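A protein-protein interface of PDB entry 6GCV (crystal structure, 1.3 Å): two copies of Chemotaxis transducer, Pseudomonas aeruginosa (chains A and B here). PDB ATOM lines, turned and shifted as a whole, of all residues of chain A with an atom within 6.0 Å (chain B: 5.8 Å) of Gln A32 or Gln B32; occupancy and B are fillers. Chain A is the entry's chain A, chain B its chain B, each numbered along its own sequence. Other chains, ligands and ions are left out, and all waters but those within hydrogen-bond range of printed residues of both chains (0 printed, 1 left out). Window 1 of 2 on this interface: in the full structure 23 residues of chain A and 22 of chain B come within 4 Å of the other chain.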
ATOM      1  N   GLN A  27     -11.576   1.517  13.240  1.00  0.00           N
ATOM      2  CA  GLN A  27     -10.540   0.662  13.831  1.00  0.00           C
ATOM      3  C   GLN A  27      -9.180   1.359  13.801  1.00  0.00           C
ATOM      4  O   GLN A  27      -8.344   1.188  14.686  1.00  0.00           O
ATOM      5  CB  GLN A  27     -10.425  -0.669  13.095  1.00  0.00           C
ATOM      6  CG  GLN A  27     -11.645  -1.573  13.119  1.00  0.00           C
ATOM      7  CD  GLN A  27     -11.974  -2.046  14.516  1.00  0.00           C
ATOM      8  OE1 GLN A  27     -12.422  -1.258  15.367  1.00  0.00           O
ATOM      9  NE2 GLN A  27     -11.789  -3.359  14.766  1.00  0.00           N
ATOM     10  N   ARG A  28      -8.912   2.070  12.707  1.00  0.00           N
ATOM     11  CA  ARG A  28      -7.664   2.808  12.566  1.00  0.00           C
ATOM     12  C   ARG A  28      -7.497   3.779  13.730  1.00  0.00           C
ATOM     13  O   ARG A  28      -6.464   3.802  14.423  1.00  0.00           O
ATOM     14  CB  ARG A  28      -7.623   3.592  11.251  1.00  0.00           C
ATOM     15  CG  ARG A  28      -7.783   2.739   9.989  1.00  0.00           C
ATOM     16  CD  ARG A  28      -7.717   3.573   8.716  1.00  0.00           C
ATOM     17  NE  ARG A  28      -8.840   4.511   8.646  1.00  0.00           N
ATOM     18  CZ  ARG A  28      -9.200   5.145   7.524  1.00  0.00           C
ATOM     19  NH1 ARG A  28      -8.576   4.888   6.387  1.00  0.00           N
ATOM     20  NH2 ARG A  28     -10.229   5.989   7.534  1.00  0.00           N
ATOM     21  N   MET A  29      -8.530   4.555  13.980  1.00  0.00           N
ATOM     22  CA  MET A  29      -8.521   5.497  15.092  1.00  0.00           C
ATOM     23  C   MET A  29      -8.359   4.780  16.431  1.00  0.00           C
ATOM     24  O   MET A  29      -7.558   5.225  17.272  1.00  0.00           O
ATOM     25  CB  MET A  29      -9.801   6.316  15.071  1.00  0.00           C
ATOM     26  CG  MET A  29      -9.937   7.326  16.188  1.00  0.00           C
ATOM     27  SD  MET A  29     -10.538   6.623  17.750  1.00  0.00           S
ATOM     28  CE  MET A  29     -12.207   6.238  17.312  1.00  0.00           C
ATOM     29  N   LEU A  30      -9.119   3.692  16.619  1.00  0.00           N
ATOM     30  CA  LEU A  30      -9.085   3.055  17.924  1.00  0.00           C
ATOM     31  C   LEU A  30      -7.687   2.533  18.245  1.00  0.00           C
ATOM     32  O   LEU A  30      -7.247   2.597  19.403  1.00  0.00           O
ATOM     33  CB  LEU A  30     -10.126   1.943  18.011  1.00  0.00           C
ATOM     34  CG  LEU A  30     -11.584   2.422  18.002  1.00  0.00           C
ATOM     35  CD1 LEU A  30     -12.520   1.270  17.752  1.00  0.00           C
ATOM     36  CD2 LEU A  30     -11.973   3.130  19.283  1.00  0.00           C
ATOM     37  N   SER A  31      -6.997   2.007  17.239  1.00  0.00           N
ATOM     38  CA  SER A  31      -5.644   1.525  17.468  1.00  0.00           C
ATOM     39  C   SER A  31      -4.736   2.602  18.048  1.00  0.00           C
ATOM     40  O   SER A  31      -3.830   2.295  18.818  1.00  0.00           O
ATOM     41  CB  SER A  31      -5.058   0.933  16.172  1.00  0.00           C
ATOM     42  OG  SER A  31      -4.634   1.926  15.234  1.00  0.00           O
ATOM     43  N   GLN A  32      -4.957   3.835  17.620  1.00  0.00           N
ATOM     44  CA  GLN A  32      -4.145   4.953  18.084  1.00  0.00           C
ATOM     45  C   GLN A  32      -4.616   5.490  19.457  1.00  0.00           C
ATOM     46  O   GLN A  32      -3.795   5.822  20.312  1.00  0.00           O
ATOM     47  CB  GLN A  32      -4.124   6.050  17.017  1.00  0.00           C
ATOM     48  CG  GLN A  32      -3.631   5.541  15.682  1.00  0.00           C
ATOM     49  CD  GLN A  32      -2.268   4.953  15.785  1.00  0.00           C
ATOM     50  OE1 GLN A  32      -1.315   5.705  15.983  1.00  0.00           O
ATOM     51  NE2 GLN A  32      -2.157   3.621  15.706  1.00  0.00           N
ATOM     52  N   LYS A  33      -5.929   5.556  19.624  1.00  0.00           N
ATOM     53  CA  LYS A  33      -6.496   5.970  20.917  1.00  0.00           C
ATOM     54  C   LYS A  33      -6.028   5.079  22.053  1.00  0.00           C
ATOM     55  O   LYS A  33      -5.661   5.565  23.134  1.00  0.00           O
ATOM     56  CB  LYS A  33      -8.031   6.025  20.818  1.00  0.00           C
ATOM     57  CG  LYS A  33      -8.730   6.532  22.080  1.00  0.00           C
ATOM     58  CD  LYS A  33     -10.208   6.776  21.805  1.00  0.00           C
ATOM     59  CE  LYS A  33     -10.893   7.417  23.001  1.00  0.00           C
ATOM     60  NZ  LYS A  33     -11.334   6.368  23.943  1.00  0.00           N
ATOM     61  N   MET A  34      -6.041   3.770  21.814  1.00  0.00           N
ATOM     62  CA  MET A  34      -5.630   2.862  22.866  1.00  0.00           C
ATOM     63  C   MET A  34      -4.144   3.046  23.192  1.00  0.00           C
ATOM     64  O   MET A  34      -3.741   2.931  24.359  1.00  0.00           O
ATOM     65  CB  MET A  34      -6.020   1.414  22.587  1.00  0.00           C
ATOM     66  CG  MET A  34      -5.400   0.833  21.384  1.00  0.00           C
ATOM     67  SD  MET A  34      -6.066  -0.803  20.983  1.00  0.00           S
ATOM     68  CE  MET A  34      -7.729  -0.627  20.367  1.00  0.00           C
ATOM     69  N   ALA A  35      -3.328   3.327  22.184  1.00  0.00           N
ATOM     70  CA  ALA A  35      -1.918   3.567  22.453  1.00  0.00           C
ATOM     71  C   ALA A  35      -1.738   4.817  23.329  1.00  0.00           C
ATOM     72  O   ALA A  35      -0.957   4.818  24.279  1.00  0.00           O
ATOM     73  CB  ALA A  35      -1.137   3.719  21.169  1.00  0.00           C
ATOM     74  N   ARG A  36      -2.438   5.888  22.992  1.00  0.00           N
ATOM     75  CA  ARG A  36      -2.331   7.059  23.818  1.00  0.00           C
ATOM     76  C   ARG A  36      -2.787   6.819  25.251  1.00  0.00           C
ATOM     77  O   ARG A  36      -2.162   7.275  26.193  1.00  0.00           O
ATOM     78  CB  ARG A  36      -2.841   8.286  23.136  1.00  0.00           C
ATOM     79  CG  ARG A  36      -4.235   8.435  22.852  1.00  0.00           C
ATOM     80  CD  ARG A  36      -4.948   9.305  23.867  1.00  0.00           C
ATOM     81  NE  ARG A  36      -6.290   9.591  23.407  1.00  0.00           N
ATOM     82  CZ  ARG A  36      -7.306  10.019  24.148  1.00  0.00           C
ATOM     83  NH1 ARG A  36      -7.264   9.911  25.464  1.00  0.00           N
ATOM     84  NH2 ARG A  36      -8.458  10.302  23.501  1.00  0.00           N
ATOM     85  N   GLU A  37      -3.880   6.083  25.412  1.00  0.00           N
ATOM     86  CA  GLU A  37      -4.364   5.773  26.762  1.00  0.00           C
ATOM     87  C   GLU A  37      -3.333   4.925  27.535  1.00  0.00           C
ATOM     88  O   GLU A  37      -3.150   5.144  28.759  1.00  0.00           O
ATOM     89  CB  GLU A  37      -5.703   5.056  26.661  1.00  0.00           C
ATOM     90  CG  GLU A  37      -6.813   5.974  26.220  1.00  0.00           C
ATOM     91  CD  GLU A  37      -8.092   5.294  25.792  1.00  0.00           C
ATOM     92  OE1 GLU A  37      -8.040   4.122  25.398  1.00  0.00           O
ATOM     93  OE2 GLU A  37      -9.179   5.946  25.797  1.00  0.00           O
ATOM     94  N   TYR A  96      -0.161  -6.853  19.598  1.00  0.00           N
ATOM     95  CA  TYR A  96      -0.275  -5.444  20.014  1.00  0.00           C
ATOM     96  C   TYR A  96      -1.037  -5.318  21.312  1.00  0.00           C
ATOM     97  O   TYR A  96      -0.654  -4.536  22.202  1.00  0.00           O
ATOM     98  CB  TYR A  96      -0.980  -4.664  18.904  1.00  0.00           C
ATOM     99  CG  TYR A  96      -1.113  -3.173  19.109  1.00  0.00           C
ATOM    100  CD1 TYR A  96       0.009  -2.347  19.212  1.00  0.00           C
ATOM    101  CD2 TYR A  96      -2.341  -2.587  19.165  1.00  0.00           C
ATOM    102  CE1 TYR A  96      -0.141  -0.964  19.349  1.00  0.00           C
ATOM    103  CE2 TYR A  96      -2.506  -1.216  19.273  1.00  0.00           C
ATOM    104  CZ  TYR A  96      -1.408  -0.401  19.333  1.00  0.00           C
ATOM    105  OH  TYR A  96      -1.536   0.982  19.352  1.00  0.00           O
ATOM    106  N   SER A 119       2.476  -0.258  16.672  1.00  0.00           N
ATOM    107  CA  SER A 119       1.272   0.557  16.508  1.00  0.00           C
ATOM    108  C   SER A 119       1.127   1.034  15.060  1.00  0.00           C
ATOM    109  O   SER A 119       0.036   0.977  14.471  1.00  0.00           O
ATOM    110  CB  SER A 119       1.320   1.761  17.456  1.00  0.00           C
ATOM    111  OG  SER A 119       0.072   2.460  17.466  1.00  0.00           O
ATOM    112  N   THR A 120       2.238   1.483  14.492  1.00  0.00           N
ATOM    113  CA  THR A 120       2.253   1.954  13.113  1.00  0.00           C
ATOM    114  C   THR A 120       1.976   0.816  12.134  1.00  0.00           C
ATOM    115  O   THR A 120       1.262   0.992  11.136  1.00  0.00           O
ATOM    116  CB  THR A 120       3.582   2.663  12.843  1.00  0.00           C
ATOM    117  OG1 THR A 120       3.601   3.843  13.661  1.00  0.00           O
ATOM    118  CG2 THR A 120       3.783   2.988  11.338  1.00  0.00           C
ATOM    119  N   LEU A 123      -1.738  -0.028  12.341  1.00  0.00           N
ATOM    120  CA  LEU A 123      -2.459   1.046  11.652  1.00  0.00           C
ATOM    121  C   LEU A 123      -2.414   0.850  10.135  1.00  0.00           C
ATOM    122  O   LEU A 123      -3.453   0.951   9.454  1.00  0.00           O
ATOM    123  CB  LEU A 123      -1.863   2.400  12.069  1.00  0.00           C
ATOM    124  CG  LEU A 123      -2.409   3.604  11.335  1.00  0.00           C
ATOM    125  CD1 LEU A 123      -3.898   3.758  11.507  1.00  0.00           C
ATOM    126  CD2 LEU A 123      -1.676   4.846  11.785  1.00  0.00           C
ATOM    127  N   GLN B  27      -9.228  11.770   9.737  1.00  0.00           N
ATOM    128  CA  GLN B  27      -8.935  12.875  10.660  1.00  0.00           C
ATOM    129  C   GLN B  27      -9.129  12.413  12.112  1.00  0.00           C
ATOM    130  O   GLN B  27      -8.393  12.839  13.022  1.00  0.00           O
ATOM    131  CB  GLN B  27      -9.843  14.072  10.413  1.00  0.00           C
ATOM    132  CG  GLN B  27      -9.673  14.772   9.052  1.00  0.00           C
ATOM    133  CD  GLN B  27      -8.317  15.404   8.897  1.00  0.00           C
ATOM    134  OE1 GLN B  27      -7.311  14.707   8.752  1.00  0.00           O
ATOM    135  NE2 GLN B  27      -8.274  16.761   8.907  1.00  0.00           N
ATOM    136  N   ARG B  28     -10.149  11.565  12.336  1.00  0.00           N
ATOM    137  CA  ARG B  28     -10.365  11.015  13.679  1.00  0.00           C
ATOM    138  C   ARG B  28      -9.082  10.310  14.142  1.00  0.00           C
ATOM    139  O   ARG B  28      -8.579  10.522  15.244  1.00  0.00           O
ATOM    140  CB  ARG B  28     -11.532  10.026  13.679  1.00  0.00           C
ATOM    141  CG  ARG B  28     -12.873  10.584  13.245  1.00  0.00           C
ATOM    142  CD  ARG B  28     -13.973   9.545  13.254  1.00  0.00           C
ATOM    143  NE  ARG B  28     -13.754   8.469  12.322  1.00  0.00           N
ATOM    144  CZ  ARG B  28     -14.680   7.602  11.925  1.00  0.00           C
ATOM    145  NH1 ARG B  28     -15.923   7.708  12.356  1.00  0.00           N
ATOM    146  NH2 ARG B  28     -14.366   6.636  11.084  1.00  0.00           N
ATOM    147  N   MET B  29      -8.596   9.413  13.310  1.00  0.00           N
ATOM    148  CA  MET B  29      -7.389   8.680  13.592  1.00  0.00           C
ATOM    149  C   MET B  29      -6.195   9.603  13.825  1.00  0.00           C
ATOM    150  O   MET B  29      -5.438   9.423  14.777  1.00  0.00           O
ATOM    151  CB  MET B  29      -7.114   7.664  12.504  1.00  0.00           C
ATOM    152  CG  MET B  29      -5.823   6.865  12.665  1.00  0.00           C
ATOM    153  SD  MET B  29      -4.324   7.717  12.158  1.00  0.00           S
ATOM    154  CE  MET B  29      -4.534   7.743  10.394  1.00  0.00           C
ATOM    155  N   LEU B  30      -6.014  10.587  12.941  1.00  0.00           N
ATOM    156  CA  LEU B  30      -4.838  11.460  13.055  1.00  0.00           C
ATOM    157  C   LEU B  30      -4.832  12.206  14.386  1.00  0.00           C
ATOM    158  O   LEU B  30      -3.780  12.393  14.982  1.00  0.00           O
ATOM    159  CB  LEU B  30      -4.743  12.408  11.872  1.00  0.00           C
ATOM    160  CG  LEU B  30      -4.452  11.735  10.528  1.00  0.00           C
ATOM    161  CD1 LEU B  30      -4.663  12.720   9.397  1.00  0.00           C
ATOM    162  CD2 LEU B  30      -3.074  11.160  10.436  1.00  0.00           C
ATOM    163  N   SER B  31      -5.994  12.644  14.844  1.00  0.00           N
ATOM    164  CA  SER B  31      -6.050  13.339  16.123  1.00  0.00           C
ATOM    165  C   SER B  31      -5.499  12.479  17.259  1.00  0.00           C
ATOM    166  O   SER B  31      -4.877  12.979  18.187  1.00  0.00           O
ATOM    167  CB  SER B  31      -7.457  13.800  16.446  1.00  0.00           C
ATOM    168  OG  SER B  31      -8.333  12.744  16.852  1.00  0.00           O
ATOM    169  N   GLN B  32      -5.738  11.174  17.173  1.00  0.00           N
ATOM    170  CA  GLN B  32      -5.288  10.257  18.205  1.00  0.00           C
ATOM    171  C   GLN B  32      -3.832   9.837  18.009  1.00  0.00           C
ATOM    172  O   GLN B  32      -3.089   9.693  18.972  1.00  0.00           O
ATOM    173  CB  GLN B  32      -6.230   9.037  18.246  1.00  0.00           C
ATOM    174  CG  GLN B  32      -7.685   9.431  18.498  1.00  0.00           C
ATOM    175  CD  GLN B  32      -7.828  10.235  19.758  1.00  0.00           C
ATOM    176  OE1 GLN B  32      -7.631   9.704  20.849  1.00  0.00           O
ATOM    177  NE2 GLN B  32      -8.075  11.550  19.631  1.00  0.00           N
ATOM    178  N   LYS B  33      -3.420   9.669  16.743  1.00  0.00           N
ATOM    179  CA  LYS B  33      -2.017   9.387  16.430  1.00  0.00           C
ATOM    180  C   LYS B  33      -1.120  10.498  16.954  1.00  0.00           C
ATOM    181  O   LYS B  33      -0.049  10.227  17.485  1.00  0.00           O
ATOM    182  CB  LYS B  33      -1.855   9.181  14.921  1.00  0.00           C
ATOM    183  CG  LYS B  33      -0.477   8.733  14.500  1.00  0.00           C
ATOM    184  CD  LYS B  33      -0.477   8.226  13.058  1.00  0.00           C
ATOM    185  CE  LYS B  33       0.860   7.721  12.604  1.00  0.00           C
ATOM    186  NZ  LYS B  33       1.694   8.854  12.115  1.00  0.00           N
ATOM    187  N   MET B  34      -1.545  11.750  16.807  1.00  0.00           N
ATOM    188  CA  MET B  34      -0.750  12.866  17.330  1.00  0.00           C
ATOM    189  C   MET B  34      -0.571  12.762  18.843  1.00  0.00           C
ATOM    190  O   MET B  34       0.508  13.058  19.363  1.00  0.00           O
ATOM    191  CB  MET B  34      -1.470  14.211  17.075  1.00  0.00           C
ATOM    192  CG  MET B  34      -1.510  14.618  15.661  1.00  0.00           C
ATOM    193  SD  MET B  34      -2.633  16.104  15.652  1.00  0.00           S
ATOM    194  CE  MET B  34      -3.321  15.746  14.013  1.00  0.00           C
ATOM    195  N   ALA B  35      -1.641  12.400  19.544  1.00  0.00           N
ATOM    196  CA  ALA B  35      -1.538  12.272  20.991  1.00  0.00           C
ATOM    197  C   ALA B  35      -0.585  11.140  21.375  1.00  0.00           C
ATOM    198  O   ALA B  35       0.214  11.285  22.294  1.00  0.00           O
ATOM    199  CB  ALA B  35      -2.898  12.045  21.588  1.00  0.00           C
ATOM    200  N   ARG B  36      -0.694  10.012  20.696  1.00  0.00           N
ATOM    201  CA  ARG B  36       0.224   8.905  20.894  1.00  0.00           C
ATOM    202  C   ARG B  36       1.672   9.372  20.706  1.00  0.00           C
ATOM    203  O   ARG B  36       2.553   9.107  21.532  1.00  0.00           O
ATOM    204  CB  ARG B  36      -0.129   7.750  19.908  1.00  0.00           C
ATOM    205  CG  ARG B  36       0.942   6.726  19.658  1.00  0.00           C
ATOM    206  CD  ARG B  36       0.776   6.075  18.307  1.00  0.00           C
ATOM    207  NE  ARG B  36       2.042   5.502  17.928  1.00  0.00           N
ATOM    208  CZ  ARG B  36       2.349   5.094  16.717  1.00  0.00           C
ATOM    209  NH1 ARG B  36       1.476   5.153  15.729  1.00  0.00           N
ATOM    210  NH2 ARG B  36       3.556   4.606  16.482  1.00  0.00           N
ATOM    211  N   GLU B  37       1.914  10.067  19.583  1.00  0.00           N
ATOM    212  CA  GLU B  37       3.268  10.537  19.306  1.00  0.00           C
ATOM    213  C   GLU B  37       3.781  11.537  20.316  1.00  0.00           C
ATOM    214  O   GLU B  37       4.956  11.509  20.691  1.00  0.00           O
ATOM    215  CB  GLU B  37       3.319  11.115  17.875  1.00  0.00           C
ATOM    216  CG  GLU B  37       3.169  10.020  16.825  1.00  0.00           C
ATOM    217  CD  GLU B  37       2.855  10.500  15.444  1.00  0.00           C
ATOM    218  OE1 GLU B  37       2.310  11.623  15.331  1.00  0.00           O
ATOM    219  OE2 GLU B  37       3.105   9.714  14.485  1.00  0.00           O
ATOM    220  N   TYR B  96      -5.909  22.416  20.472  1.00  0.00           N
ATOM    221  CA  TYR B  96      -5.283  21.106  20.624  1.00  0.00           C
ATOM    222  C   TYR B  96      -3.863  21.104  20.102  1.00  0.00           C
ATOM    223  O   TYR B  96      -2.946  20.519  20.720  1.00  0.00           O
ATOM    224  CB  TYR B  96      -6.126  20.075  19.912  1.00  0.00           C
ATOM    225  CG  TYR B  96      -5.660  18.643  20.017  1.00  0.00           C
ATOM    226  CD1 TYR B  96      -5.697  17.990  21.251  1.00  0.00           C
ATOM    227  CD2 TYR B  96      -5.267  17.923  18.921  1.00  0.00           C
ATOM    228  CE1 TYR B  96      -5.369  16.660  21.348  1.00  0.00           C
ATOM    229  CE2 TYR B  96      -4.981  16.585  19.001  1.00  0.00           C
ATOM    230  CZ  TYR B  96      -5.020  15.954  20.234  1.00  0.00           C
ATOM    231  OH  TYR B  96      -4.784  14.596  20.327  1.00  0.00           O
ATOM    232  N   SER B 119      -8.310  15.845  23.770  1.00  0.00           N
ATOM    233  CA  SER B 119      -8.138  14.920  22.651  1.00  0.00           C
ATOM    234  C   SER B 119      -9.445  14.201  22.340  1.00  0.00           C
ATOM    235  O   SER B 119      -9.826  14.053  21.183  1.00  0.00           O
ATOM    236  CB  SER B 119      -7.034  13.899  22.990  1.00  0.00           C
ATOM    237  OG  SER B 119      -6.713  13.089  21.869  1.00  0.00           O
ATOM    238  N   THR B 120     -10.124  13.752  23.390  1.00  0.00           N
ATOM    239  CA  THR B 120     -11.407  13.081  23.232  1.00  0.00           C
ATOM    240  C   THR B 120     -12.485  14.030  22.711  1.00  0.00           C
ATOM    241  O   THR B 120     -13.329  13.649  21.901  1.00  0.00           O
ATOM    242  CB  THR B 120     -11.766  12.353  24.517  1.00  0.00           C
ATOM    243  OG1 THR B 120     -10.793  11.305  24.696  1.00  0.00           O
ATOM    244  CG2 THR B 120     -13.147  11.761  24.467  1.00  0.00           C
ATOM    245  N   LEU B 123     -11.796  14.482  18.999  1.00  0.00           N
ATOM    246  CA  LEU B 123     -12.223  13.230  18.364  1.00  0.00           C
ATOM    247  C   LEU B 123     -13.743  13.217  18.180  1.00  0.00           C
ATOM    248  O   LEU B 123     -14.256  12.854  17.110  1.00  0.00           O
ATOM    249  CB  LEU B 123     -11.762  12.049  19.203  1.00  0.00           C
ATOM    250  CG  LEU B 123     -12.270  10.687  18.775  1.00  0.00           C
ATOM    251  CD1 LEU B 123     -11.876  10.345  17.376  1.00  0.00           C
ATOM    252  CD2 LEU B 123     -11.772   9.627  19.759  1.00  0.00           C
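The side-chain amide oxygen of Gln A32 is in hydrogen-bond range of the guanidinium group of Arg B36 (2.9 Å). OG of Ser A119 lies within hydrogen-bond range of NH1 of Arg B36 (3.5 Å). OG1 of Thr A120 is in hydrogen-bond range of NH2 of Arg B36. The side-chain hydroxyl (OG1) of Thr B120 lies within hydrogen-bond range of the guanidinium group (NH2) of Arg A36 (2.8 Å). The guanidinium group (NH2) of Arg A36 lies within hydrogen-bond range of the side-chain amide oxygen (OE1) of Gln B32 (2.8 Å).
NE2 of Gln A32 lies within hydrogen-bond range of OG of Ser A31, at 3.0 Å. O of Arg B28 is in hydrogen-bond range of OG of Ser B31 (2.8 Å). The side-chain amide nitrogen of Gln A32 is in hydrogen-bond range of the side-chain hydroxyl of Ser A119 (3.1 Å). OH of Tyr A96 is in hydrogen-bond range of OG of Ser A119. The side-chain amide nitrogen (NE2) of Gln B32 lies within hydrogen-bond range of the side-chain hydroxyl (OG) of Ser B119. NZ of Lys B33 lies within salt-bridge range of OE2 of Glu B37 (2.9 Å).
Among the printed residues, merely in contact across the chains: Arg A28 with Met B29 (3.6 Å), Met A29 with Arg B28 (3.6 Å), Met A29 with Met B29 (3.7 Å), Met A29 with Gln B32 (3.9 Å), Met A29 with Leu B123 (3.8 Å), Gln A32 with Met B29 (3.96 Å), Gln A32 with Gln B32 (3.9 Å), Gln A32 with Lys B33 (3.5 Å), Lys A33 with Gln B32 (3.6 Å), Lys A33 with Leu B123 (3.8 Å), Ala A35 with Arg B36 (3.96 Å), Arg A36 with Arg B36 (3.7 Å), Arg A36 with Ser B119 (3.7 Å), Leu A123 with Met B29 (3.8 Å) and Leu A123 with Lys B33 (3.8 Å).
Gln B32 touches just these residues of chain A: Met A29 (3.9 Å), Gln A32 (3.9 Å), Lys A33 (3.6 Å) and Arg A36 (2.8 Å). Of the printed residues of chain A, Lys B33 touches Gln A32 and Leu A123. Printed residues of chain B within 4 Å of Leu A123: Met B29 and Lys B33. Of the printed residues of chain B, Lys A33 touches Gln B32 and Leu B123. Printed residues of chain B within 4 Å of Ser A119: Arg B36 (3.5 Å). Of the printed residues of chain B, Thr A120 touches Arg B36. Ala B35 touches none of the printed residues of chain A. Tyr A96 touches none of the printed residues of chain B. The nearest printed residue of chain B that does not touch Gln A32 is Met B34 (6.1 Å). The nearest printed residue of chain A that does not touch Gln B32 is Leu A30 (6.2 Å).
Of the 15 printed residues of chain A, 9 touch a printed residue of chain B. Printed residues of chain A that touch a printed residue of chain B: Arg A28, Met A29, Gln A32, Lys A33, Ala A35, Arg A36, Ser A119, Thr A120 and Leu A123. Hydrophobic or aromatic side chains of chain A that line the printed part of chain B: Met A29, Ala A35 and Leu A123. Of the 15 printed residues of chain B, 8 touch a printed residue of chain A.
Arg A28 touches Met B29, and with the chains exchanged Met A29 touches Arg B28. Met B29 touches its own counterpart, Met A29. Met A29 touches Gln B32, and with the chains exchanged Gln A32 touches Met B29. Met A29 touches Leu B123, and with the chains exchanged Leu A123 touches Met B29. Of the 20 pairs that touch across the chains among the printed residues, 19 have their exchanged pair printed and touching as well.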
